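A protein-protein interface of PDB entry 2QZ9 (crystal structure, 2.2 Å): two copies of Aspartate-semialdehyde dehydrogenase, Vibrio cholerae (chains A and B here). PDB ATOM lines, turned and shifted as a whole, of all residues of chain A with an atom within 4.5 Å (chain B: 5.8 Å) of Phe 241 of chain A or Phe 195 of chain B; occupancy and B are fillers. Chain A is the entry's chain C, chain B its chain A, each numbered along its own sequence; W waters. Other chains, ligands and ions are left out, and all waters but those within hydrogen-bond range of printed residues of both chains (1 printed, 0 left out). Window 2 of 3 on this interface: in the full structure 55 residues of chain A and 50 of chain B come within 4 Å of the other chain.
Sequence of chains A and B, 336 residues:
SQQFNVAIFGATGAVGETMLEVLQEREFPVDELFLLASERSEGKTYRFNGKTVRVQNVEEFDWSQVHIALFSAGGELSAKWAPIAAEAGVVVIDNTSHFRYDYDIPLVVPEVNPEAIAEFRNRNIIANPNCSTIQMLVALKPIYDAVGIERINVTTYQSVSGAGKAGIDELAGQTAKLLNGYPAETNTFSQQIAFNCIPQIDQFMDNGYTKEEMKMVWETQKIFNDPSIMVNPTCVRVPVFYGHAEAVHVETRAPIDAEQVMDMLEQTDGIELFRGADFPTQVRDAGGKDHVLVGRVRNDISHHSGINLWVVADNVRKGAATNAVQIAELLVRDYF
Water W1 bridges O of Phe 195 of chain B (2.7 Å) and N of Phe 241 of chain A (3.0 Å).
The side-chain amide oxygen of Asn 196 of chain B lies within hydrogen-bond range of the backbone NH of Val 283 of chain A, at 2.9 Å.
O of Leu 171 of chain A lies within hydrogen-bond range of OG1 of Thr 175 of chain A, 2.8 Å away.
The side-chain amide oxygen of Gln 192 of chain B sits close to the backbone carbonyl oxygen of Ala 194 of chain B, at 2.9 Å.
The backbone carbonyl oxygen of Gln 192 of chain B sits at hydrogen-bond distance from the side-chain amide nitrogen of Asn 196 of chain B (2.8 Å).
The side-chain hydroxyl of Ser 161 of chain A lies within hydrogen-bond range of the backbone carbonyl oxygen of Phe 241 of chain A.
The backbone carbonyl oxygen (O) of Leu 171 of chain B lies within hydrogen-bond range of the side-chain hydroxyl (OG1) of Thr 175 of chain B.
O of Val 240 of chain A lies within hydrogen-bond range of N of Val 160 of chain A (2.9 Å).
Thr 175 of chain B touches its own counterpart, Thr 175 of chain A.
Pro 239 of chain B touches its own counterpart, Pro 239 of chain A.
Positions printed for both chains: 171, 175 and 239.
Of the 11 pairs that touch across the chains among the printed residues, 2 have their exchanged pair printed and touching as well.
Of the printed residues of chain B, Pro 239 of chain A touches Phe 195 and Pro 239.
Phe 241 of chain A touches one residue of chain B.
Printed residues of chain A within 4 Å of Leu 179 of chain B: Thr 175.
Of chain A, only Pro 239 (3.2 Å), Val 240 (3.5 Å), Phe 241 (3.6 Å) and Val 283 (2.9 Å) come within 4 Å of Phe 195 of chain B.
Printed residues of chain A within 4 Å of Cys 197 of chain B: Val 240 (3.9 Å).
The nearest residue of chain B that does not touch Phe 241 of chain A is Leu 179 of chain B (5.4 Å).
The nearest residue of chain A that does not touch Phe 195 of chain B is Leu 171 of chain A (4.1 Å).
The nearest printed residue of chain A that does not touch Gln 192 of chain B is Phe 241 of chain A (7.9 Å).
Thr 175 of chain A touches Thr 175 of chain B.
Thr 175 of chain A touches Leu 179 of chain B (CG2 to CD1, 3.8 Å).
Phe 195 of chain B touches Pro 239 of chain A.
CD of Pro 239 of chain B touches CD of Pro 239 of chain A (3.8 Å).
Phe 195 of chain B touches Val 240 of chain A (O to CG2, 3.5 Å).
Val 240 of chain A touches Asn 196 of chain B (CG2 to N, 3.7 Å).
Val 240 of chain A touches Cys 197 of chain B.
CE1 of Phe 241 of chain A touches CE2 of Phe 195 of chain B (3.6 Å).
Gln 192 of chain B touches Val 283 of chain A (NE2 to CG1, 3.4 Å).
Val 283 of chain A touches Phe 195 of chain B (CG2 to O, 2.9 Å).
Hydrophobic or aromatic side chains of chain B that line the printed part of chain A: Leu 179, Phe 195 and Pro 239.
Along chain B the printed residues that touch a printed residue of chain A span positions 175 to 239.
Hydrophobic or aromatic side chains of chain A within 4 Å of the printed part of chain B: Pro 239, Val 240, Phe 241 and Val 283.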
ATOM      1  N   SER A 159     -10.447  20.355  -9.734  1.00  0.00           N
ATOM      2  CA  SER A 159     -10.412  21.711 -10.309  1.00  0.00           C
ATOM      3  C   SER A 159     -11.220  22.734  -9.511  1.00  0.00           C
ATOM      4  O   SER A 159     -12.124  22.376  -8.743  1.00  0.00           O
ATOM      5  CB  SER A 159     -10.919  21.684 -11.745  1.00  0.00           C
ATOM      6  OG  SER A 159     -12.257  21.242 -11.764  1.00  0.00           O
ATOM      7  N   VAL A 160     -10.883  24.005  -9.696  1.00  0.00           N
ATOM      8  CA  VAL A 160     -11.495  25.105  -8.942  1.00  0.00           C
ATOM      9  C   VAL A 160     -12.985  25.278  -9.263  1.00  0.00           C
ATOM     10  O   VAL A 160     -13.724  25.847  -8.469  1.00  0.00           O
ATOM     11  CB  VAL A 160     -10.747  26.437  -9.145  1.00  0.00           C
ATOM     12  CG1 VAL A 160      -9.328  26.339  -8.579  1.00  0.00           C
ATOM     13  CG2 VAL A 160     -10.721  26.841 -10.621  1.00  0.00           C
ATOM     14  N   SER A 161     -13.426  24.753 -10.405  1.00  0.00           N
ATOM     15  CA  SER A 161     -14.818  24.896 -10.822  1.00  0.00           C
ATOM     16  C   SER A 161     -15.732  24.105  -9.884  1.00  0.00           C
ATOM     17  O   SER A 161     -16.936  24.349  -9.842  1.00  0.00           O
ATOM     18  CB  SER A 161     -15.019  24.477 -12.272  1.00  0.00           C
ATOM     19  OG  SER A 161     -14.667  23.120 -12.460  1.00  0.00           O
ATOM     20  N   ILE A 168     -13.323  29.758  -9.992  1.00  0.00           N
ATOM     21  CA  ILE A 168     -12.726  30.118 -11.277  1.00  0.00           C
ATOM     22  C   ILE A 168     -12.136  31.532 -11.258  1.00  0.00           C
ATOM     23  O   ILE A 168     -10.973  31.728 -11.632  1.00  0.00           O
ATOM     24  CB  ILE A 168     -13.745  29.941 -12.429  1.00  0.00           C
ATOM     25  CG1 ILE A 168     -14.081  28.458 -12.582  1.00  0.00           C
ATOM     26  CG2 ILE A 168     -13.194  30.507 -13.745  1.00  0.00           C
ATOM     27  CD1 ILE A 168     -15.358  28.169 -13.342  1.00  0.00           C
ATOM     28  N   LEU A 171      -8.983  31.730  -9.272  1.00  0.00           N
ATOM     29  CA  LEU A 171      -7.807  31.179  -9.951  1.00  0.00           C
ATOM     30  C   LEU A 171      -7.319  32.076 -11.088  1.00  0.00           C
ATOM     31  O   LEU A 171      -6.160  32.472 -11.092  1.00  0.00           O
ATOM     32  CB  LEU A 171      -8.035  29.747 -10.463  1.00  0.00           C
ATOM     33  CG  LEU A 171      -6.836  29.107 -11.199  1.00  0.00           C
ATOM     34  CD1 LEU A 171      -5.605  28.986 -10.305  1.00  0.00           C
ATOM     35  CD2 LEU A 171      -7.179  27.770 -11.808  1.00  0.00           C
ATOM     36  N   ALA A 172      -8.197  32.368 -12.051  1.00  0.00           N
ATOM     37  CA  ALA A 172      -7.882  33.285 -13.150  1.00  0.00           C
ATOM     38  C   ALA A 172      -7.413  34.615 -12.593  1.00  0.00           C
ATOM     39  O   ALA A 172      -6.484  35.221 -13.122  1.00  0.00           O
ATOM     40  CB  ALA A 172      -9.086  33.477 -14.057  1.00  0.00           C
ATOM     41  N   THR A 175      -3.755  34.303 -10.600  1.00  0.00           N
ATOM     42  CA  THR A 175      -2.719  33.938 -11.563  1.00  0.00           C
ATOM     43  C   THR A 175      -2.280  35.163 -12.374  1.00  0.00           C
ATOM     44  O   THR A 175      -1.082  35.420 -12.501  1.00  0.00           O
ATOM     45  CB  THR A 175      -3.179  32.785 -12.480  1.00  0.00           C
ATOM     46  OG1 THR A 175      -3.517  31.650 -11.676  1.00  0.00           O
ATOM     47  CG2 THR A 175      -2.079  32.378 -13.445  1.00  0.00           C
ATOM     48  N   PRO A 239      -4.640  23.797  -9.144  1.00  0.00           N
ATOM     49  CA  PRO A 239      -4.846  25.040  -9.909  1.00  0.00           C
ATOM     50  C   PRO A 239      -5.201  24.747 -11.360  1.00  0.00           C
ATOM     51  O   PRO A 239      -4.472  25.087 -12.297  1.00  0.00           O
ATOM     52  CB  PRO A 239      -3.502  25.785  -9.770  1.00  0.00           C
ATOM     53  CG  PRO A 239      -2.523  24.796  -9.131  1.00  0.00           C
ATOM     54  CD  PRO A 239      -3.211  23.444  -9.077  1.00  0.00           C
ATOM     55  N   VAL A 240      -6.341  24.088 -11.500  1.00  0.00           N
ATOM     56  CA  VAL A 240      -6.889  23.677 -12.762  1.00  0.00           C
ATOM     57  C   VAL A 240      -8.293  24.273 -12.804  1.00  0.00           C
ATOM     58  O   VAL A 240      -8.909  24.441 -11.745  1.00  0.00           O
ATOM     59  CB  VAL A 240      -6.927  22.138 -12.814  1.00  0.00           C
ATOM     60  CG1 VAL A 240      -7.709  21.614 -14.005  1.00  0.00           C
ATOM     61  CG2 VAL A 240      -5.491  21.579 -12.800  1.00  0.00           C
ATOM     62  N   PHE A 241      -8.788  24.586 -14.012  1.00  0.00           N
ATOM     63  CA  PHE A 241     -10.150  25.128 -14.190  1.00  0.00           C
ATOM     64  C   PHE A 241     -11.257  24.074 -14.253  1.00  0.00           C
ATOM     65  O   PHE A 241     -12.162  24.105 -13.427  1.00  0.00           O
ATOM     66  CB  PHE A 241     -10.236  26.085 -15.402  1.00  0.00           C
ATOM     67  CG  PHE A 241      -9.583  27.410 -15.165  1.00  0.00           C
ATOM     68  CD1 PHE A 241      -8.391  27.734 -15.797  1.00  0.00           C
ATOM     69  CD2 PHE A 241     -10.144  28.328 -14.283  1.00  0.00           C
ATOM     70  CE1 PHE A 241      -7.770  28.954 -15.573  1.00  0.00           C
ATOM     71  CE2 PHE A 241      -9.526  29.553 -14.047  1.00  0.00           C
ATOM     72  CZ  PHE A 241      -8.339  29.866 -14.697  1.00  0.00           C
ATOM     73  N   TYR A 242     -11.191  23.154 -15.219  1.00  0.00           N
ATOM     74  CA  TYR A 242     -12.258  22.156 -15.433  1.00  0.00           C
ATOM     75  C   TYR A 242     -11.780  20.691 -15.420  1.00  0.00           C
ATOM     76  O   TYR A 242     -10.660  20.388 -15.833  1.00  0.00           O
ATOM     77  CB  TYR A 242     -13.045  22.463 -16.729  1.00  0.00           C
ATOM     78  CG  TYR A 242     -13.346  23.946 -16.863  1.00  0.00           C
ATOM     79  CD1 TYR A 242     -14.359  24.549 -16.107  1.00  0.00           C
ATOM     80  CD2 TYR A 242     -12.572  24.756 -17.695  1.00  0.00           C
ATOM     81  CE1 TYR A 242     -14.610  25.928 -16.208  1.00  0.00           C
ATOM     82  CE2 TYR A 242     -12.809  26.127 -17.801  1.00  0.00           C
ATOM     83  CZ  TYR A 242     -13.822  26.704 -17.054  1.00  0.00           C
ATOM     84  OH  TYR A 242     -14.045  28.057 -17.176  1.00  0.00           O
ATOM     85  N   VAL A 283      -7.037  19.291 -18.907  1.00  0.00           N
ATOM     86  CA  VAL A 283      -7.016  20.290 -19.987  1.00  0.00           C
ATOM     87  C   VAL A 283      -7.143  19.673 -21.384  1.00  0.00           C
ATOM     88  O   VAL A 283      -7.829  20.222 -22.261  1.00  0.00           O
ATOM     89  CB  VAL A 283      -5.738  21.173 -19.925  1.00  0.00           C
ATOM     90  CG1 VAL A 283      -5.572  22.017 -21.193  1.00  0.00           C
ATOM     91  CG2 VAL A 283      -5.778  22.074 -18.727  1.00  0.00           C
ATOM     92  N   LEU B 171       6.096  26.282 -17.474  1.00  0.00           N
ATOM     93  CA  LEU B 171       4.929  26.656 -16.679  1.00  0.00           C
ATOM     94  C   LEU B 171       4.596  28.138 -16.828  1.00  0.00           C
ATOM     95  O   LEU B 171       3.494  28.469 -17.252  1.00  0.00           O
ATOM     96  CB  LEU B 171       5.085  26.287 -15.192  1.00  0.00           C
ATOM     97  CG  LEU B 171       3.902  26.657 -14.276  1.00  0.00           C
ATOM     98  CD1 LEU B 171       2.561  26.077 -14.774  1.00  0.00           C
ATOM     99  CD2 LEU B 171       4.163  26.258 -12.830  1.00  0.00           C
ATOM    100  N   THR B 175       1.527  29.641 -19.229  1.00  0.00           N
ATOM    101  CA  THR B 175       0.469  30.283 -18.450  1.00  0.00           C
ATOM    102  C   THR B 175       0.175  31.692 -18.978  1.00  0.00           C
ATOM    103  O   THR B 175      -0.990  32.092 -19.058  1.00  0.00           O
ATOM    104  CB  THR B 175       0.790  30.274 -16.920  1.00  0.00           C
ATOM    105  OG1 THR B 175       1.002  28.925 -16.483  1.00  0.00           O
ATOM    106  CG2 THR B 175      -0.351  30.862 -16.106  1.00  0.00           C
ATOM    107  N   LEU B 178      -1.490  31.391 -22.559  1.00  0.00           N
ATOM    108  CA  LEU B 178      -2.901  31.023 -22.398  1.00  0.00           C
ATOM    109  C   LEU B 178      -3.777  32.172 -21.901  1.00  0.00           C
ATOM    110  O   LEU B 178      -4.874  32.382 -22.425  1.00  0.00           O
ATOM    111  CB  LEU B 178      -3.064  29.795 -21.501  1.00  0.00           C
ATOM    112  CG  LEU B 178      -2.634  28.462 -22.118  1.00  0.00           C
ATOM    113  CD1 LEU B 178      -2.456  27.414 -21.030  1.00  0.00           C
ATOM    114  CD2 LEU B 178      -3.588  27.981 -23.214  1.00  0.00           C
ATOM    115  N   LEU B 179      -3.290  32.914 -20.908  1.00  0.00           N
ATOM    116  CA  LEU B 179      -4.058  34.021 -20.338  1.00  0.00           C
ATOM    117  C   LEU B 179      -4.256  35.171 -21.325  1.00  0.00           C
ATOM    118  O   LEU B 179      -5.330  35.774 -21.370  1.00  0.00           O
ATOM    119  CB  LEU B 179      -3.438  34.523 -19.030  1.00  0.00           C
ATOM    120  CG  LEU B 179      -3.566  33.649 -17.772  1.00  0.00           C
ATOM    121  CD1 LEU B 179      -3.048  34.407 -16.562  1.00  0.00           C
ATOM    122  CD2 LEU B 179      -4.992  33.157 -17.526  1.00  0.00           C
ATOM    123  N   GLN B 192       0.312  19.629 -21.874  1.00  0.00           N
ATOM    124  CA  GLN B 192       0.323  20.978 -21.301  1.00  0.00           C
ATOM    125  C   GLN B 192       0.306  20.889 -19.778  1.00  0.00           C
ATOM    126  O   GLN B 192      -0.441  20.085 -19.210  1.00  0.00           O
ATOM    127  CB  GLN B 192      -0.899  21.756 -21.799  1.00  0.00           C
ATOM    128  CG  GLN B 192      -1.062  23.167 -21.238  1.00  0.00           C
ATOM    129  CD  GLN B 192      -2.450  23.748 -21.509  1.00  0.00           C
ATOM    130  OE1 GLN B 192      -3.082  24.320 -20.613  1.00  0.00           O
ATOM    131  NE2 GLN B 192      -2.935  23.592 -22.743  1.00  0.00           N
ATOM    132  N   ILE B 193       1.129  21.710 -19.129  1.00  0.00           N
ATOM    133  CA  ILE B 193       1.227  21.714 -17.676  1.00  0.00           C
ATOM    134  C   ILE B 193       0.418  22.840 -17.025  1.00  0.00           C
ATOM    135  O   ILE B 193      -0.207  22.631 -15.976  1.00  0.00           O
ATOM    136  CB  ILE B 193       2.715  21.724 -17.171  1.00  0.00           C
ATOM    137  CG1 ILE B 193       2.786  21.541 -15.646  1.00  0.00           C
ATOM    138  CG2 ILE B 193       3.431  22.997 -17.579  1.00  0.00           C
ATOM    139  CD1 ILE B 193       2.057  20.298 -15.122  1.00  0.00           C
ATOM    140  N   ALA B 194       0.445  24.026 -17.635  1.00  0.00           N
ATOM    141  CA  ALA B 194      -0.318  25.164 -17.143  1.00  0.00           C
ATOM    142  C   ALA B 194      -1.777  24.749 -16.951  1.00  0.00           C
ATOM    143  O   ALA B 194      -2.383  24.167 -17.848  1.00  0.00           O
ATOM    144  CB  ALA B 194      -0.210  26.339 -18.122  1.00  0.00           C
ATOM    145  N   PHE B 195      -2.313  25.013 -15.761  1.00  0.00           N
ATOM    146  CA  PHE B 195      -3.690  24.612 -15.388  1.00  0.00           C
ATOM    147  C   PHE B 195      -4.006  23.140 -15.658  1.00  0.00           C
ATOM    148  O   PHE B 195      -5.138  22.804 -16.039  1.00  0.00           O
ATOM    149  CB  PHE B 195      -4.741  25.475 -16.104  1.00  0.00           C
ATOM    150  CG  PHE B 195      -4.476  26.943 -16.049  1.00  0.00           C
ATOM    151  CD1 PHE B 195      -4.241  27.657 -17.226  1.00  0.00           C
ATOM    152  CD2 PHE B 195      -4.483  27.625 -14.838  1.00  0.00           C
ATOM    153  CE1 PHE B 195      -4.003  29.037 -17.189  1.00  0.00           C
ATOM    154  CE2 PHE B 195      -4.243  28.996 -14.792  1.00  0.00           C
ATOM    155  CZ  PHE B 195      -3.998  29.704 -15.972  1.00  0.00           C
ATOM    156  N   ASN B 196      -3.012  22.271 -15.464  1.00  0.00           N
ATOM    157  CA  ASN B 196      -3.170  20.845 -15.740  1.00  0.00           C
ATOM    158  C   ASN B 196      -2.353  19.980 -14.768  1.00  0.00           C
ATOM    159  O   ASN B 196      -1.447  20.470 -14.096  1.00  0.00           O
ATOM    160  CB  ASN B 196      -2.780  20.535 -17.193  1.00  0.00           C
ATOM    161  CG  ASN B 196      -3.495  19.321 -17.760  1.00  0.00           C
ATOM    162  OD1 ASN B 196      -4.578  18.952 -17.317  1.00  0.00           O
ATOM    163  ND2 ASN B 196      -2.895  18.709 -18.774  1.00  0.00           N
ATOM    164  N   CYS B 197      -2.687  18.695 -14.703  1.00  0.00           N
ATOM    165  CA  CYS B 197      -1.937  17.733 -13.895  1.00  0.00           C
ATOM    166  C   CYS B 197      -1.547  16.626 -14.840  1.00  0.00           C
ATOM    167  O   CYS B 197      -2.377  16.147 -15.610  1.00  0.00           O
ATOM    168  CB  CYS B 197      -2.779  17.192 -12.717  1.00  0.00           C
ATOM    169  SG  CYS B 197      -3.365  18.488 -11.586  1.00  0.00           S
ATOM    170  N   PRO B 239       0.900  22.226 -11.510  1.00  0.00           N
ATOM    171  CA  PRO B 239       1.289  23.577 -11.950  1.00  0.00           C
ATOM    172  C   PRO B 239       1.732  24.462 -10.799  1.00  0.00           C
ATOM    173  O   PRO B 239       1.182  25.541 -10.582  1.00  0.00           O
ATOM    174  CB  PRO B 239       0.005  24.133 -12.602  1.00  0.00           C
ATOM    175  CG  PRO B 239      -1.037  23.047 -12.474  1.00  0.00           C
ATOM    176  CD  PRO B 239      -0.564  22.094 -11.436  1.00  0.00           C
HETATM  177  O   HOH W   1      -7.530  23.979 -16.689  1.00  0.00           O
